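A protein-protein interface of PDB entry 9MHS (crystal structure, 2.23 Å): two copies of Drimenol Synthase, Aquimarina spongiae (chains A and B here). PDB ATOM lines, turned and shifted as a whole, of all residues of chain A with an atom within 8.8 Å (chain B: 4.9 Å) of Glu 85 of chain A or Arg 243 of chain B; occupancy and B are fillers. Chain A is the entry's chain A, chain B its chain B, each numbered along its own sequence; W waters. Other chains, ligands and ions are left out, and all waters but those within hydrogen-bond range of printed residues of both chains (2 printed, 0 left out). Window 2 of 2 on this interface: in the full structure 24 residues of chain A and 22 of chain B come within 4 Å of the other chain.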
ATOM      1  N   LYS A  58     -26.554  -3.231  20.702  1.00  0.00           N
ATOM      2  CA  LYS A  58     -26.410  -1.781  20.670  1.00  0.00           C
ATOM      3  C   LYS A  58     -25.255  -1.327  21.553  1.00  0.00           C
ATOM      4  O   LYS A  58     -24.668  -0.266  21.316  1.00  0.00           O
ATOM      5  CB  LYS A  58     -27.717  -1.112  21.100  1.00  0.00           C
ATOM      6  N   HIS A  62     -21.270   0.135  19.942  1.00  0.00           N
ATOM      7  CA  HIS A  62     -20.982   1.529  20.247  1.00  0.00           C
ATOM      8  C   HIS A  62     -19.475   1.774  20.220  1.00  0.00           C
ATOM      9  O   HIS A  62     -18.701   0.900  20.618  1.00  0.00           O
ATOM     10  CB  HIS A  62     -21.549   1.897  21.619  1.00  0.00           C
ATOM     11  CG  HIS A  62     -21.563   3.366  21.886  1.00  0.00           C
ATOM     12  ND1 HIS A  62     -20.455   4.049  22.338  1.00  0.00           N
ATOM     13  CD2 HIS A  62     -22.548   4.287  21.761  1.00  0.00           C
ATOM     14  CE1 HIS A  62     -20.757   5.328  22.481  1.00  0.00           C
ATOM     15  NE2 HIS A  62     -22.020   5.498  22.136  1.00  0.00           N
ATOM     16  N   PRO A  63     -19.028   2.942  19.740  1.00  0.00           N
ATOM     17  CA  PRO A  63     -17.574   3.208  19.708  1.00  0.00           C
ATOM     18  C   PRO A  63     -16.891   3.041  21.063  1.00  0.00           C
ATOM     19  O   PRO A  63     -15.747   2.573  21.122  1.00  0.00           O
ATOM     20  CB  PRO A  63     -17.496   4.658  19.198  1.00  0.00           C
ATOM     21  CG  PRO A  63     -18.774   4.869  18.438  1.00  0.00           C
ATOM     22  CD  PRO A  63     -19.809   4.049  19.152  1.00  0.00           C
ATOM     23  N   VAL A  64     -17.564   3.401  22.158  1.00  0.00           N
ATOM     24  CA  VAL A  64     -16.956   3.259  23.479  1.00  0.00           C
ATOM     25  C   VAL A  64     -16.603   1.803  23.751  1.00  0.00           C
ATOM     26  O   VAL A  64     -15.562   1.499  24.345  1.00  0.00           O
ATOM     27  CB  VAL A  64     -17.888   3.831  24.562  1.00  0.00           C
ATOM     28  CG1 VAL A  64     -17.458   3.371  25.953  1.00  0.00           C
ATOM     29  CG2 VAL A  64     -17.892   5.346  24.488  1.00  0.00           C
ATOM     30  N   ALA A  78     -16.394   2.084  31.092  1.00  0.00           N
ATOM     31  CA  ALA A  78     -17.135   1.902  29.843  1.00  0.00           C
ATOM     32  C   ALA A  78     -18.645   1.824  30.082  1.00  0.00           C
ATOM     33  O   ALA A  78     -19.438   2.318  29.270  1.00  0.00           O
ATOM     34  CB  ALA A  78     -16.647   0.645  29.122  1.00  0.00           C
ATOM     35  N   LEU A  79     -19.062   1.185  31.179  1.00  0.00           N
ATOM     36  CA  LEU A  79     -20.482   1.130  31.496  1.00  0.00           C
ATOM     37  C   LEU A  79     -20.994   2.488  31.945  1.00  0.00           C
ATOM     38  O   LEU A  79     -22.145   2.837  31.668  1.00  0.00           O
ATOM     39  CB  LEU A  79     -20.750   0.076  32.570  1.00  0.00           C
ATOM     40  CG  LEU A  79     -20.607  -1.393  32.152  1.00  0.00           C
ATOM     41  CD1 LEU A  79     -20.849  -2.344  33.327  1.00  0.00           C
ATOM     42  CD2 LEU A  79     -21.558  -1.709  31.019  1.00  0.00           C
ATOM     43  N   THR A  80     -20.164   3.263  32.643  1.00  0.00           N
ATOM     44  CA  THR A  80     -20.575   4.610  33.021  1.00  0.00           C
ATOM     45  C   THR A  80     -20.869   5.439  31.778  1.00  0.00           C
ATOM     46  O   THR A  80     -21.934   6.058  31.668  1.00  0.00           O
ATOM     47  CB  THR A  80     -19.501   5.291  33.876  1.00  0.00           C
ATOM     48  OG1 THR A  80     -19.260   4.525  35.057  1.00  0.00           O
ATOM     49  CG2 THR A  80     -19.942   6.690  34.275  1.00  0.00           C
ATOM     50  N   ALA A  81     -19.942   5.441  30.818  1.00  0.00           N
ATOM     51  CA  ALA A  81     -20.157   6.219  29.605  1.00  0.00           C
ATOM     52  C   ALA A  81     -21.379   5.713  28.850  1.00  0.00           C
ATOM     53  O   ALA A  81     -22.289   6.486  28.527  1.00  0.00           O
ATOM     54  CB  ALA A  81     -18.909   6.178  28.719  1.00  0.00           C
ATOM     55  N   LEU A  82     -21.430   4.403  28.603  1.00  0.00           N
ATOM     56  CA  LEU A  82     -22.526   3.812  27.850  1.00  0.00           C
ATOM     57  C   LEU A  82     -23.849   3.988  28.566  1.00  0.00           C
ATOM     58  O   LEU A  82     -24.899   4.016  27.915  1.00  0.00           O
ATOM     59  CB  LEU A  82     -22.229   2.334  27.585  1.00  0.00           C
ATOM     60  CG  LEU A  82     -21.115   2.121  26.548  1.00  0.00           C
ATOM     61  CD1 LEU A  82     -20.594   0.685  26.494  1.00  0.00           C
ATOM     62  CD2 LEU A  82     -21.603   2.560  25.183  1.00  0.00           C
ATOM     63  N   SER A  83     -23.818   4.142  29.887  1.00  0.00           N
ATOM     64  CA  SER A  83     -25.041   4.456  30.613  1.00  0.00           C
ATOM     65  C   SER A  83     -25.619   5.780  30.140  1.00  0.00           C
ATOM     66  O   SER A  83     -26.840   5.930  30.018  1.00  0.00           O
ATOM     67  CB  SER A  83     -24.758   4.494  32.112  1.00  0.00           C
ATOM     68  OG  SER A  83     -25.778   5.197  32.777  1.00  0.00           O
ATOM     69  N   CYS A  84     -24.744   6.742  29.852  1.00  0.00           N
ATOM     70  CA  CYS A  84     -25.168   8.048  29.365  1.00  0.00           C
ATOM     71  C   CYS A  84     -25.606   7.983  27.900  1.00  0.00           C
ATOM     72  O   CYS A  84     -26.699   8.439  27.545  1.00  0.00           O
ATOM     73  CB  CYS A  84     -24.018   9.043  29.557  1.00  0.00           C
ATOM     74  SG  CYS A  84     -24.222  10.666  28.791  1.00  0.00           S
ATOM     75  N   GLU A  85     -24.770   7.418  27.033  1.00  0.00           N
ATOM     76  CA  GLU A  85     -25.092   7.420  25.609  1.00  0.00           C
ATOM     77  C   GLU A  85     -26.298   6.543  25.305  1.00  0.00           C
ATOM     78  O   GLU A  85     -27.141   6.906  24.480  1.00  0.00           O
ATOM     79  CB  GLU A  85     -23.879   6.972  24.795  1.00  0.00           C
ATOM     80  CG  GLU A  85     -22.655   7.786  25.125  1.00  0.00           C
ATOM     81  CD  GLU A  85     -22.960   9.274  25.110  1.00  0.00           C
ATOM     82  OE1 GLU A  85     -23.467   9.749  24.083  1.00  0.00           O
ATOM     83  OE2 GLU A  85     -22.724   9.963  26.126  1.00  0.00           O
ATOM     84  N   LEU A  86     -26.415   5.398  25.969  1.00  0.00           N
ATOM     85  CA  LEU A  86     -27.530   4.505  25.702  1.00  0.00           C
ATOM     86  C   LEU A  86     -28.759   4.820  26.544  1.00  0.00           C
ATOM     87  O   LEU A  86     -29.777   4.139  26.385  1.00  0.00           O
ATOM     88  CB  LEU A  86     -27.095   3.057  25.922  1.00  0.00           C
ATOM     89  CG  LEU A  86     -25.832   2.795  25.119  1.00  0.00           C
ATOM     90  CD1 LEU A  86     -25.220   1.424  25.437  1.00  0.00           C
ATOM     91  CD2 LEU A  86     -26.156   2.945  23.644  1.00  0.00           C
ATOM     92  N   GLU A  87     -28.694   5.835  27.416  1.00  0.00           N
ATOM     93  CA  GLU A  87     -29.828   6.262  28.249  1.00  0.00           C
ATOM     94  C   GLU A  87     -30.464   5.063  28.946  1.00  0.00           C
ATOM     95  O   GLU A  87     -31.680   4.849  28.909  1.00  0.00           O
ATOM     96  CB  GLU A  87     -30.861   7.029  27.429  1.00  0.00           C
ATOM     97  CG  GLU A  87     -30.254   8.199  26.698  1.00  0.00           C
ATOM     98  CD  GLU A  87     -31.258   8.974  25.884  1.00  0.00           C
ATOM     99  OE1 GLU A  87     -32.424   9.106  26.326  1.00  0.00           O
ATOM    100  OE2 GLU A  87     -30.873   9.450  24.795  1.00  0.00           O
ATOM    101  N   THR A  88     -29.610   4.267  29.578  1.00  0.00           N
ATOM    102  CA  THR A  88     -29.982   3.050  30.256  1.00  0.00           C
ATOM    103  C   THR A  88     -29.265   3.069  31.599  1.00  0.00           C
ATOM    104  O   THR A  88     -28.072   3.412  31.651  1.00  0.00           O
ATOM    105  CB  THR A  88     -29.574   1.822  29.436  1.00  0.00           C
ATOM    106  OG1 THR A  88     -30.221   1.860  28.154  1.00  0.00           O
ATOM    107  CG2 THR A  88     -29.916   0.523  30.178  1.00  0.00           C
ATOM    108  N   LEU A  93     -27.221  -2.225  32.090  1.00  0.00           N
ATOM    109  CA  LEU A  93     -26.192  -2.614  31.118  1.00  0.00           C
ATOM    110  C   LEU A  93     -25.294  -3.703  31.684  1.00  0.00           C
ATOM    111  O   LEU A  93     -24.879  -4.612  30.956  1.00  0.00           O
ATOM    112  CB  LEU A  93     -25.333  -1.414  30.692  1.00  0.00           C
ATOM    113  CG  LEU A  93     -25.973  -0.239  29.945  1.00  0.00           C
ATOM    114  CD1 LEU A  93     -24.922   0.796  29.558  1.00  0.00           C
ATOM    115  CD2 LEU A  93     -26.742  -0.710  28.716  1.00  0.00           C
ATOM    116  N   TYR B 239     -19.487  15.447  19.166  1.00  0.00           N
ATOM    117  CA  TYR B 239     -20.079  14.869  20.363  1.00  0.00           C
ATOM    118  C   TYR B 239     -20.845  15.922  21.162  1.00  0.00           C
ATOM    119  O   TYR B 239     -22.037  15.753  21.459  1.00  0.00           O
ATOM    120  CB  TYR B 239     -18.995  14.201  21.220  1.00  0.00           C
ATOM    121  CG  TYR B 239     -19.584  13.656  22.486  1.00  0.00           C
ATOM    122  CD1 TYR B 239     -20.163  12.392  22.510  1.00  0.00           C
ATOM    123  CD2 TYR B 239     -19.610  14.420  23.643  1.00  0.00           C
ATOM    124  CE1 TYR B 239     -20.728  11.900  23.652  1.00  0.00           C
ATOM    125  CE2 TYR B 239     -20.170  13.935  24.797  1.00  0.00           C
ATOM    126  CZ  TYR B 239     -20.732  12.674  24.788  1.00  0.00           C
ATOM    127  OH  TYR B 239     -21.308  12.193  25.922  1.00  0.00           O
ATOM    128  N   LEU B 240     -20.187  17.029  21.508  1.00  0.00           N
ATOM    129  CA  LEU B 240     -20.833  17.985  22.404  1.00  0.00           C
ATOM    130  C   LEU B 240     -22.005  18.680  21.720  1.00  0.00           C
ATOM    131  O   LEU B 240     -23.037  18.927  22.357  1.00  0.00           O
ATOM    132  CB  LEU B 240     -19.825  19.013  22.927  1.00  0.00           C
ATOM    133  CG  LEU B 240     -20.277  19.980  24.044  1.00  0.00           C
ATOM    134  CD1 LEU B 240     -20.758  19.234  25.291  1.00  0.00           C
ATOM    135  CD2 LEU B 240     -19.150  20.948  24.416  1.00  0.00           C
ATOM    136  N   ASN B 241     -21.867  18.999  20.425  1.00  0.00           N
ATOM    137  CA  ASN B 241     -22.959  19.655  19.706  1.00  0.00           C
ATOM    138  C   ASN B 241     -24.205  18.776  19.683  1.00  0.00           C
ATOM    139  O   ASN B 241     -25.319  19.259  19.903  1.00  0.00           O
ATOM    140  CB  ASN B 241     -22.536  20.001  18.273  1.00  0.00           C
ATOM    141  CG  ASN B 241     -21.525  21.133  18.207  1.00  0.00           C
ATOM    142  OD1 ASN B 241     -21.291  21.850  19.178  1.00  0.00           O
ATOM    143  ND2 ASN B 241     -20.919  21.296  17.047  1.00  0.00           N
ATOM    144  N   LEU B 242     -24.030  17.482  19.422  1.00  0.00           N
ATOM    145  CA  LEU B 242     -25.169  16.582  19.420  1.00  0.00           C
ATOM    146  C   LEU B 242     -25.754  16.427  20.817  1.00  0.00           C
ATOM    147  O   LEU B 242     -26.980  16.436  20.973  1.00  0.00           O
ATOM    148  CB  LEU B 242     -24.776  15.225  18.840  1.00  0.00           C
ATOM    149  CG  LEU B 242     -25.995  14.300  18.772  1.00  0.00           C
ATOM    150  CD1 LEU B 242     -27.064  14.927  17.900  1.00  0.00           C
ATOM    151  CD2 LEU B 242     -25.657  12.877  18.293  1.00  0.00           C
ATOM    152  N   ARG B 243     -24.900  16.309  21.848  1.00  0.00           N
ATOM    153  CA  ARG B 243     -25.404  16.162  23.218  1.00  0.00           C
ATOM    154  C   ARG B 243     -26.178  17.400  23.653  1.00  0.00           C
ATOM    155  O   ARG B 243     -27.266  17.289  24.237  1.00  0.00           O
ATOM    156  CB  ARG B 243     -24.261  15.889  24.205  1.00  0.00           C
ATOM    157  CG  ARG B 243     -23.540  14.554  24.040  1.00  0.00           C
ATOM    158  CD  ARG B 243     -24.414  13.364  24.447  1.00  0.00           C
ATOM    159  NE  ARG B 243     -24.972  13.515  25.790  1.00  0.00           N
ATOM    160  CZ  ARG B 243     -25.818  12.660  26.350  1.00  0.00           C
ATOM    161  NH1 ARG B 243     -26.157  11.536  25.750  1.00  0.00           N
ATOM    162  NH2 ARG B 243     -26.341  12.945  27.543  1.00  0.00           N
ATOM    163  N   LEU B 244     -25.629  18.589  23.391  1.00  0.00           N
ATOM    164  CA  LEU B 244     -26.302  19.809  23.818  1.00  0.00           C
ATOM    165  C   LEU B 244     -27.519  20.119  22.950  1.00  0.00           C
ATOM    166  O   LEU B 244     -28.448  20.780  23.418  1.00  0.00           O
ATOM    167  CB  LEU B 244     -25.322  20.983  23.823  1.00  0.00           C
ATOM    168  CG  LEU B 244     -24.230  20.826  24.897  1.00  0.00           C
ATOM    169  CD1 LEU B 244     -23.217  21.973  24.850  1.00  0.00           C
ATOM    170  CD2 LEU B 244     -24.876  20.702  26.287  1.00  0.00           C
ATOM    171  N   ARG B 245     -27.534  19.666  21.691  1.00  0.00           N
ATOM    172  CA  ARG B 245     -28.739  19.815  20.880  1.00  0.00           C
ATOM    173  C   ARG B 245     -29.863  18.948  21.420  1.00  0.00           C
ATOM    174  O   ARG B 245     -30.988  19.423  21.596  1.00  0.00           O
ATOM    175  CB  ARG B 245     -28.456  19.478  19.416  1.00  0.00           C
ATOM    176  CG  ARG B 245     -27.921  20.653  18.664  1.00  0.00           C
ATOM    177  CD  ARG B 245     -27.297  20.271  17.333  1.00  0.00           C
ATOM    178  NE  ARG B 245     -26.883  21.484  16.645  1.00  0.00           N
ATOM    179  CZ  ARG B 245     -26.003  21.529  15.658  1.00  0.00           C
ATOM    180  NH1 ARG B 245     -25.464  20.426  15.159  1.00  0.00           N
ATOM    181  NH2 ARG B 245     -25.643  22.714  15.170  1.00  0.00           N
ATOM    182  N   LYS B 246     -29.573  17.675  21.701  1.00  0.00           N
ATOM    183  CA  LYS B 246     -30.600  16.781  22.224  1.00  0.00           C
ATOM    184  C   LYS B 246     -31.017  17.180  23.636  1.00  0.00           C
ATOM    185  O   LYS B 246     -32.205  17.098  23.984  1.00  0.00           O
ATOM    186  CB  LYS B 246     -30.112  15.327  22.196  1.00  0.00           C
ATOM    187  N   PHE B 247     -30.068  17.642  24.453  1.00  0.00           N
ATOM    188  CA  PHE B 247     -30.322  17.946  25.862  1.00  0.00           C
ATOM    189  C   PHE B 247     -29.796  19.334  26.195  1.00  0.00           C
ATOM    190  O   PHE B 247     -28.757  19.484  26.854  1.00  0.00           O
ATOM    191  CB  PHE B 247     -29.703  16.880  26.767  1.00  0.00           C
ATOM    192  CG  PHE B 247     -30.139  15.484  26.426  1.00  0.00           C
ATOM    193  CD1 PHE B 247     -31.413  15.053  26.739  1.00  0.00           C
ATOM    194  CD2 PHE B 247     -29.279  14.609  25.774  1.00  0.00           C
ATOM    195  CE1 PHE B 247     -31.818  13.772  26.422  1.00  0.00           C
ATOM    196  CE2 PHE B 247     -29.681  13.325  25.454  1.00  0.00           C
ATOM    197  CZ  PHE B 247     -30.951  12.903  25.776  1.00  0.00           C
ATOM    198  N   PRO B 248     -30.501  20.383  25.751  1.00  0.00           N
ATOM    199  CA  PRO B 248     -29.989  21.739  25.963  1.00  0.00           C
ATOM    200  C   PRO B 248     -30.032  22.159  27.411  1.00  0.00           C
ATOM    201  O   PRO B 248     -29.248  23.034  27.806  1.00  0.00           O
ATOM    202  CB  PRO B 248     -30.909  22.603  25.086  1.00  0.00           C
ATOM    203  CG  PRO B 248     -32.169  21.815  25.002  1.00  0.00           C
ATOM    204  CD  PRO B 248     -31.752  20.382  24.979  1.00  0.00           C
ATOM    205  N   LYS B 251     -27.627  17.903  31.002  1.00  0.00           N
ATOM    206  CA  LYS B 251     -27.837  16.780  31.897  1.00  0.00           C
ATOM    207  C   LYS B 251     -26.813  16.783  33.038  1.00  0.00           C
ATOM    208  O   LYS B 251     -25.794  17.484  32.999  1.00  0.00           O
ATOM    209  CB  LYS B 251     -27.766  15.473  31.113  1.00  0.00           C
ATOM    210  CG  LYS B 251     -28.964  15.258  30.195  1.00  0.00           C
ATOM    211  CD  LYS B 251     -28.944  13.870  29.580  1.00  0.00           C
ATOM    212  CE  LYS B 251     -29.422  12.814  30.567  1.00  0.00           C
ATOM    213  NZ  LYS B 251     -30.895  12.892  30.784  1.00  0.00           N
ATOM    214  N   ASP B 490     -16.135   8.035  20.996  1.00  0.00           N
ATOM    215  CA  ASP B 490     -17.255   8.808  20.469  1.00  0.00           C
ATOM    216  C   ASP B 490     -17.022  10.315  20.523  1.00  0.00           C
ATOM    217  O   ASP B 490     -17.930  11.072  20.182  1.00  0.00           O
ATOM    218  CB  ASP B 490     -18.543   8.455  21.224  1.00  0.00           C
ATOM    219  CG  ASP B 490     -18.461   8.745  22.728  1.00  0.00           C
ATOM    220  OD1 ASP B 490     -17.389   9.149  23.245  1.00  0.00           O
ATOM    221  OD2 ASP B 490     -19.498   8.565  23.398  1.00  0.00           O
ATOM    222  N   ARG B 511     -20.633  14.151  31.087  1.00  0.00           N
ATOM    223  CA  ARG B 511     -19.706  14.149  29.968  1.00  0.00           C
ATOM    224  C   ARG B 511     -19.735  15.474  29.207  1.00  0.00           C
ATOM    225  O   ARG B 511     -18.720  15.879  28.630  1.00  0.00           O
ATOM    226  CB  ARG B 511     -20.038  12.990  29.047  1.00  0.00           C
ATOM    227  CG  ARG B 511     -19.933  11.628  29.739  1.00  0.00           C
ATOM    228  CD  ARG B 511     -20.054  10.507  28.712  1.00  0.00           C
ATOM    229  NE  ARG B 511     -18.900  10.484  27.819  1.00  0.00           N
ATOM    230  CZ  ARG B 511     -18.836   9.817  26.672  1.00  0.00           C
ATOM    231  NH1 ARG B 511     -19.876   9.151  26.198  1.00  0.00           N
ATOM    232  NH2 ARG B 511     -17.695   9.807  25.991  1.00  0.00           N
ATOM    233  N   GLU B 512     -20.877  16.164  29.206  1.00  0.00           N
ATOM    234  CA  GLU B 512     -20.959  17.464  28.552  1.00  0.00           C
ATOM    235  C   GLU B 512     -20.013  18.457  29.208  1.00  0.00           C
ATOM    236  O   GLU B 512     -19.271  19.166  28.523  1.00  0.00           O
ATOM    237  CB  GLU B 512     -22.395  17.997  28.586  1.00  0.00           C
ATOM    238  CG  GLU B 512     -23.366  17.280  27.683  1.00  0.00           C
ATOM    239  CD  GLU B 512     -23.988  16.051  28.318  1.00  0.00           C
ATOM    240  OE1 GLU B 512     -23.417  15.494  29.284  1.00  0.00           O
ATOM    241  OE2 GLU B 512     -25.066  15.636  27.849  1.00  0.00           O
HETATM  242  O   HOH W   1     -23.126  12.990  30.765  1.00  0.00           O
HETATM  243  O   HOH W   2     -22.125   8.508  21.979  1.00  0.00           O
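Printed residues of chain B within 4 Å of Glu 85 of chain A: Tyr 239 (2.6 Å), Arg 243 (3.6 Å), Asp 490 (3.7 Å) and Arg 511 (3.0 Å).
Of chain A, only Cys 84 and Glu 85 come within 4 Å of Arg 243 of chain B.
Of the printed residues of chain A, Phe 247 of chain B touches Glu 87.
Printed residues of chain B within 4 Å of His 62 of chain A: Asp 490 (3.6 Å).
Printed residues of chain B within 4 Å of Glu 87 of chain A: Phe 247.
Lys 246 of chain B touches none of the printed residues of chain A.
Leu 244 of chain B touches none of the printed residues of chain A.
The nearest printed residue of chain B that does not touch Glu 85 of chain A is Glu 512 of chain B (6.4 Å).
No position is printed for both chains.
Of the 8 pairs that touch across the chains among the printed residues, none has its exchanged pair printed and touching as well.
NH1 of Arg 243 of chain B lies within salt-bridge range of OE1 of Glu 85 of chain A, at 3.6 Å.
The guanidinium group (NH2) of Arg 243 of chain B lies within hydrogen-bond range of the side-chain sulfur (SG) of Cys 84 of chain A (3.4 Å).
The side-chain hydroxyl (OH) of Tyr 239 of chain B sits at hydrogen-bond distance from the side-chain carboxylate (OE2) of Glu 85 of chain A (2.6 Å).
The guanidinium group (NH1) of Arg 511 of chain B lies within salt-bridge range of the side-chain carboxylate (OE2) of Glu 85 of chain A.
Printed residues of chain B that touch a printed residue of chain A: Tyr 239, Arg 243, Phe 247, Asp 490 and Arg 511.
Hydrophobic or aromatic side chains of chain B within 4 Å of the printed part of chain A: Tyr 239 and Phe 247.
Of the 16 printed residues of chain A, 5 touch a printed residue of chain B.
Hydrophobic or aromatic side chains of chain A within 4 Å of the printed part of chain B: His 62 and Val 64.
Among the printed residues, Asp or Glu carboxylates within 4 Å of a Lys or Arg side-chain nitrogen of the other chain: Glu 85 of chain A with Arg 243 of chain B and Glu 85 of chain A with Arg 511 of chain B.
OD1 of Asp 490 of chain B lies within salt-bridge range of NH2 of Arg 511 of chain B (2.8 Å).
SG of Cys 84 of chain A sits at hydrogen-bond distance from OE2 of Glu 85 of chain A (3.1 Å).
The side-chain hydroxyl of Tyr 239 of chain B lies within hydrogen-bond range of the guanidinium group of Arg 511 of chain B.
The guanidinium group (NE) of Arg 243 of chain B lies within salt-bridge range of the side-chain carboxylate (OE2) of Glu 512 of chain B (3.0 Å).
A ring nitrogen (ND1) of His 62 of chain A lies within hydrogen-bond range of the backbone NH (N) of Val 64 of chain A (3.0 Å).
Water W1 lies within hydrogen-bond range of N of Arg 511 of chain B (2.8 Å), OE1 of Glu 512 of chain B (2.9 Å) and SG of Cys 84 of chain A (3.2 Å).
Water W2 lies within hydrogen-bond range of OE1 of Glu 85 of chain A (2.8 Å), OD2 of Asp 490 of chain B (3.0 Å) and NE2 of His 62 of chain A (3.0 Å).
Among the printed residues, pairs that only touch across the chains: Glu 87 of chain A with Phe 247 of chain B (3.6 Å), His 62 of chain A with Asp 490 of chain B (3.6 Å), Glu 85 of chain A with Asp 490 of chain B (3.7 Å) and Val 64 of chain A with Asp 490 of chain B (3.8 Å).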
